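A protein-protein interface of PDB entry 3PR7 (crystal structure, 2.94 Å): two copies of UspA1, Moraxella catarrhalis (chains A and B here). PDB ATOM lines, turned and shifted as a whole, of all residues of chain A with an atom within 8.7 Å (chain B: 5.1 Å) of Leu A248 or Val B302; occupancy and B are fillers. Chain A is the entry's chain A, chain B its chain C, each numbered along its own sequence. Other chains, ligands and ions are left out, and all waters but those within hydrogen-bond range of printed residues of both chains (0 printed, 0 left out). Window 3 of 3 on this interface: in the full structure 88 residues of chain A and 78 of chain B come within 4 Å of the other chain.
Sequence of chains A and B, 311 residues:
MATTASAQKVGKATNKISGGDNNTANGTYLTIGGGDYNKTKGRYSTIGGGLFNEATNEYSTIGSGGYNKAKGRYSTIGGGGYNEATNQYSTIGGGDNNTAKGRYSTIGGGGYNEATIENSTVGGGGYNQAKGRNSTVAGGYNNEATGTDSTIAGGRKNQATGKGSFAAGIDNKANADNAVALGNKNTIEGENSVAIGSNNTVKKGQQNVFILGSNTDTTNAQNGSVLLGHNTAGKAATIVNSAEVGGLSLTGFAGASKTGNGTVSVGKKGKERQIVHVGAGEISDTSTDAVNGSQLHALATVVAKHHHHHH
The backbone NH (N) of Leu A250 sits at hydrogen-bond distance from the backbone carbonyl oxygen (O) of Ala A243 (2.8 Å).
Among the printed residues, merely in contact across the chains: Leu A248 with Val B302 (3.97 Å), Leu A250 with Ala B298 (3.8 Å), Leu A250 with Leu B299 (3.9 Å), Leu A250 with Val B302 (3.9 Å), Leu A299 with Leu B299 (3.8 Å) and Leu A299 with Ala B300 (3.98 Å).
Leu A248 touches just one residue of chain B: Val B302.
Val B302 touches just these residues of chain A: Leu A248 and Leu A250.
No residue of chain A comes within 4 Å of Thr B301.
Printed residues of chain B within 4 Å of Leu A299: Leu B299 and Ala B300.
Printed residues of chain A within 4 Å of Ala B300: Leu A299 (3.98 Å).
Of the printed residues of chain A, Ala B298 touches Leu A250 (3.8 Å).
Of the printed residues of chain B, Leu A250 touches Ala B298 (3.8 Å), Leu B299 (3.9 Å) and Val B302 (3.9 Å).
Printed residues of chain A within 4 Å of Leu B299: Leu A250 and Leu A299.
Ser A249 touches none of the printed residues of chain B.
The nearest residue of chain B that does not touch Leu A248 is Leu B299 (4.8 Å).
The nearest residue of chain A that does not touch Val B302 is Ser A249 (5.1 Å).
Of the 7 printed residues of chain B, 4 touch a printed residue of chain A.
Printed residues of chain B that touch a printed residue of chain A: Ala B298, Leu B299, Ala B300 and Val B302.
Hydrophobic or aromatic side chains of chain B within 4 Å of the printed part of chain A: Leu B299, Ala B300 and Val B302.
Hydrophobic or aromatic side chains of chain A within 4 Å of the printed part of chain B: Leu A248, Leu A250 and Leu A299.
Among the printed residues, no Asp or Glu carboxylate lies within 4 Å of a Lys or Arg side-chain nitrogen of the other chain.
Leu A299 touches its own counterpart, Leu B299.
Positions printed for both chains: 299 and 303.
Of the 6 pairs that touch across the chains among the printed residues, 1 has its exchanged pair printed and touching as well.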
ATOM      1  N   SER A 242     -17.998  24.207  -4.065  1.00  0.00           N
ATOM      2  CA  SER A 242     -18.840  24.090  -2.883  1.00  0.00           C
ATOM      3  C   SER A 242     -18.237  24.834  -1.693  1.00  0.00           C
ATOM      4  O   SER A 242     -17.120  25.354  -1.775  1.00  0.00           O
ATOM      5  CB  SER A 242     -19.056  22.612  -2.536  1.00  0.00           C
ATOM      6  OG  SER A 242     -17.824  21.948  -2.315  1.00  0.00           O
ATOM      7  N   ALA A 243     -18.989  24.890  -0.597  1.00  0.00           N
ATOM      8  CA  ALA A 243     -18.516  25.477   0.654  1.00  0.00           C
ATOM      9  C   ALA A 243     -19.121  24.747   1.848  1.00  0.00           C
ATOM     10  O   ALA A 243     -20.154  24.084   1.720  1.00  0.00           O
ATOM     11  CB  ALA A 243     -18.852  26.957   0.707  1.00  0.00           C
ATOM     12  N   GLU A 244     -18.472  24.864   3.003  1.00  0.00           N
ATOM     13  CA  GLU A 244     -18.985  24.271   4.236  1.00  0.00           C
ATOM     14  C   GLU A 244     -19.025  25.265   5.390  1.00  0.00           C
ATOM     15  O   GLU A 244     -18.008  25.860   5.749  1.00  0.00           O
ATOM     16  CB  GLU A 244     -18.190  23.024   4.627  1.00  0.00           C
ATOM     17  CG  GLU A 244     -18.490  21.808   3.760  1.00  0.00           C
ATOM     18  CD  GLU A 244     -18.764  20.550   4.571  1.00  0.00           C
ATOM     19  OE1 GLU A 244     -18.571  20.565   5.806  1.00  0.00           O
ATOM     20  OE2 GLU A 244     -19.183  19.540   3.969  1.00  0.00           O
ATOM     21  N   VAL A 245     -20.215  25.440   5.957  1.00  0.00           N
ATOM     22  CA  VAL A 245     -20.416  26.332   7.095  1.00  0.00           C
ATOM     23  C   VAL A 245     -20.967  25.531   8.275  1.00  0.00           C
ATOM     24  O   VAL A 245     -22.164  25.238   8.337  1.00  0.00           O
ATOM     25  CB  VAL A 245     -21.367  27.515   6.751  1.00  0.00           C
ATOM     26  CG1 VAL A 245     -21.452  28.497   7.911  1.00  0.00           C
ATOM     27  CG2 VAL A 245     -20.909  28.236   5.491  1.00  0.00           C
ATOM     28  N   GLY A 246     -20.072  25.173   9.194  1.00  0.00           N
ATOM     29  CA  GLY A 246     -20.431  24.453  10.416  1.00  0.00           C
ATOM     30  C   GLY A 246     -21.309  23.236  10.203  1.00  0.00           C
ATOM     31  O   GLY A 246     -22.449  23.195  10.672  1.00  0.00           O
ATOM     32  N   GLY A 247     -20.783  22.249   9.482  1.00  0.00           N
ATOM     33  CA  GLY A 247     -21.499  20.999   9.238  1.00  0.00           C
ATOM     34  C   GLY A 247     -22.445  21.038   8.053  1.00  0.00           C
ATOM     35  O   GLY A 247     -22.748  20.002   7.462  1.00  0.00           O
ATOM     36  N   LEU A 248     -22.918  22.234   7.713  1.00  0.00           N
ATOM     37  CA  LEU A 248     -23.792  22.435   6.562  1.00  0.00           C
ATOM     38  C   LEU A 248     -22.967  22.653   5.298  1.00  0.00           C
ATOM     39  O   LEU A 248     -22.127  23.554   5.246  1.00  0.00           O
ATOM     40  CB  LEU A 248     -24.727  23.628   6.803  1.00  0.00           C
ATOM     41  CG  LEU A 248     -25.569  24.187   5.649  1.00  0.00           C
ATOM     42  CD1 LEU A 248     -26.629  23.193   5.185  1.00  0.00           C
ATOM     43  CD2 LEU A 248     -26.212  25.502   6.060  1.00  0.00           C
ATOM     44  N   SER A 249     -23.210  21.823   4.286  1.00  0.00           N
ATOM     45  CA  SER A 249     -22.508  21.934   3.011  1.00  0.00           C
ATOM     46  C   SER A 249     -23.404  22.515   1.921  1.00  0.00           C
ATOM     47  O   SER A 249     -24.581  22.162   1.818  1.00  0.00           O
ATOM     48  CB  SER A 249     -21.949  20.579   2.570  1.00  0.00           C
ATOM     49  OG  SER A 249     -22.990  19.666   2.281  1.00  0.00           O
ATOM     50  N   LEU A 250     -22.829  23.409   1.121  1.00  0.00           N
ATOM     51  CA  LEU A 250     -23.525  24.037   0.003  1.00  0.00           C
ATOM     52  C   LEU A 250     -22.822  23.677  -1.297  1.00  0.00           C
ATOM     53  O   LEU A 250     -21.714  24.145  -1.555  1.00  0.00           O
ATOM     54  CB  LEU A 250     -23.555  25.555   0.179  1.00  0.00           C
ATOM     55  CG  LEU A 250     -24.253  26.122   1.416  1.00  0.00           C
ATOM     56  CD1 LEU A 250     -23.818  27.559   1.659  1.00  0.00           C
ATOM     57  CD2 LEU A 250     -25.765  26.029   1.280  1.00  0.00           C
ATOM     58  N   THR A 251     -23.470  22.847  -2.109  1.00  0.00           N
ATOM     59  CA  THR A 251     -22.854  22.304  -3.322  1.00  0.00           C
ATOM     60  C   THR A 251     -23.543  22.772  -4.603  1.00  0.00           C
ATOM     61  O   THR A 251     -24.672  23.267  -4.570  1.00  0.00           O
ATOM     62  CB  THR A 251     -22.843  20.752  -3.310  1.00  0.00           C
ATOM     63  OG1 THR A 251     -24.179  20.263  -3.143  1.00  0.00           O
ATOM     64  CG2 THR A 251     -21.961  20.217  -2.184  1.00  0.00           C
ATOM     65  N   LEU A 299     -33.773  37.008   1.136  1.00  0.00           N
ATOM     66  CA  LEU A 299     -33.582  35.711   1.785  1.00  0.00           C
ATOM     67  C   LEU A 299     -33.478  35.830   3.307  1.00  0.00           C
ATOM     68  O   LEU A 299     -34.048  35.014   4.032  1.00  0.00           O
ATOM     69  CB  LEU A 299     -32.362  34.982   1.212  1.00  0.00           C
ATOM     70  CG  LEU A 299     -32.124  33.537   1.670  1.00  0.00           C
ATOM     71  CD1 LEU A 299     -33.270  32.615   1.277  1.00  0.00           C
ATOM     72  CD2 LEU A 299     -30.816  33.010   1.120  1.00  0.00           C
ATOM     73  N   VAL A 303     -35.465  34.253   6.887  1.00  0.00           N
ATOM     74  CA  VAL A 303     -34.749  33.679   8.034  1.00  0.00           C
ATOM     75  C   VAL A 303     -35.181  34.313   9.377  1.00  0.00           C
ATOM     76  O   VAL A 303     -34.581  34.052  10.421  1.00  0.00           O
ATOM     77  CB  VAL A 303     -33.200  33.699   7.820  1.00  0.00           C
ATOM     78  CG1 VAL A 303     -32.477  32.920   8.913  1.00  0.00           C
ATOM     79  CG2 VAL A 303     -32.844  33.100   6.466  1.00  0.00           C
ATOM     80  N   ALA B 298     -28.180  28.105  -3.900  1.00  0.00           N
ATOM     81  CA  ALA B 298     -27.731  26.994  -3.063  1.00  0.00           C
ATOM     82  C   ALA B 298     -28.223  27.133  -1.623  1.00  0.00           C
ATOM     83  O   ALA B 298     -28.770  26.182  -1.056  1.00  0.00           O
ATOM     84  CB  ALA B 298     -26.216  26.873  -3.105  1.00  0.00           C
ATOM     85  N   LEU B 299     -28.047  28.323  -1.047  1.00  0.00           N
ATOM     86  CA  LEU B 299     -28.498  28.597   0.318  1.00  0.00           C
ATOM     87  C   LEU B 299     -30.025  28.605   0.439  1.00  0.00           C
ATOM     88  O   LEU B 299     -30.574  28.069   1.404  1.00  0.00           O
ATOM     89  CB  LEU B 299     -27.900  29.909   0.844  1.00  0.00           C
ATOM     90  CG  LEU B 299     -28.146  30.246   2.323  1.00  0.00           C
ATOM     91  CD1 LEU B 299     -27.537  29.203   3.261  1.00  0.00           C
ATOM     92  CD2 LEU B 299     -27.615  31.627   2.652  1.00  0.00           C
ATOM     93  N   ALA B 300     -30.697  29.206  -0.542  1.00  0.00           N
ATOM     94  CA  ALA B 300     -32.161  29.262  -0.577  1.00  0.00           C
ATOM     95  C   ALA B 300     -32.799  27.871  -0.630  1.00  0.00           C
ATOM     96  O   ALA B 300     -33.862  27.652  -0.043  1.00  0.00           O
ATOM     97  CB  ALA B 300     -32.634  30.111  -1.749  1.00  0.00           C
ATOM     98  N   THR B 301     -32.141  26.946  -1.331  1.00  0.00           N
ATOM     99  CA  THR B 301     -32.566  25.544  -1.405  1.00  0.00           C
ATOM    100  C   THR B 301     -32.706  24.942  -0.008  1.00  0.00           C
ATOM    101  O   THR B 301     -33.701  24.282   0.294  1.00  0.00           O
ATOM    102  CB  THR B 301     -31.575  24.693  -2.245  1.00  0.00           C
ATOM    103  OG1 THR B 301     -31.493  25.221  -3.570  1.00  0.00           O
ATOM    104  CG2 THR B 301     -32.021  23.238  -2.332  1.00  0.00           C
ATOM    105  N   VAL B 302     -31.706  25.191   0.836  1.00  0.00           N
ATOM    106  CA  VAL B 302     -31.693  24.713   2.218  1.00  0.00           C
ATOM    107  C   VAL B 302     -32.829  25.337   3.034  1.00  0.00           C
ATOM    108  O   VAL B 302     -33.392  24.688   3.917  1.00  0.00           O
ATOM    109  CB  VAL B 302     -30.320  24.975   2.896  1.00  0.00           C
ATOM    110  CG1 VAL B 302     -30.298  24.449   4.327  1.00  0.00           C
ATOM    111  CG2 VAL B 302     -29.197  24.335   2.087  1.00  0.00           C
ATOM    112  N   VAL B 303     -33.180  26.580   2.716  1.00  0.00           N
ATOM    113  CA  VAL B 303     -34.265  27.282   3.413  1.00  0.00           C
ATOM    114  C   VAL B 303     -35.659  26.731   3.034  1.00  0.00           C
ATOM    115  O   VAL B 303     -36.687  27.304   3.400  1.00  0.00           O
ATOM    116  CB  VAL B 303     -34.158  28.829   3.234  1.00  0.00           C
ATOM    117  CG1 VAL B 303     -35.161  29.559   4.118  1.00  0.00           C
ATOM    118  CG2 VAL B 303     -32.753  29.308   3.574  1.00  0.00           C
ATOM    119  N   ALA B 304     -35.686  25.613   2.312  1.00  0.00           N
ATOM    120  CA  ALA B 304     -36.922  24.850   2.123  1.00  0.00           C
ATOM    121  C   ALA B 304     -37.003  23.714   3.151  1.00  0.00           C
ATOM    122  O   ALA B 304     -36.567  22.588   2.899  1.00  0.00           O
ATOM    123  CB  ALA B 304     -37.021  24.313   0.698  1.00  0.00           C
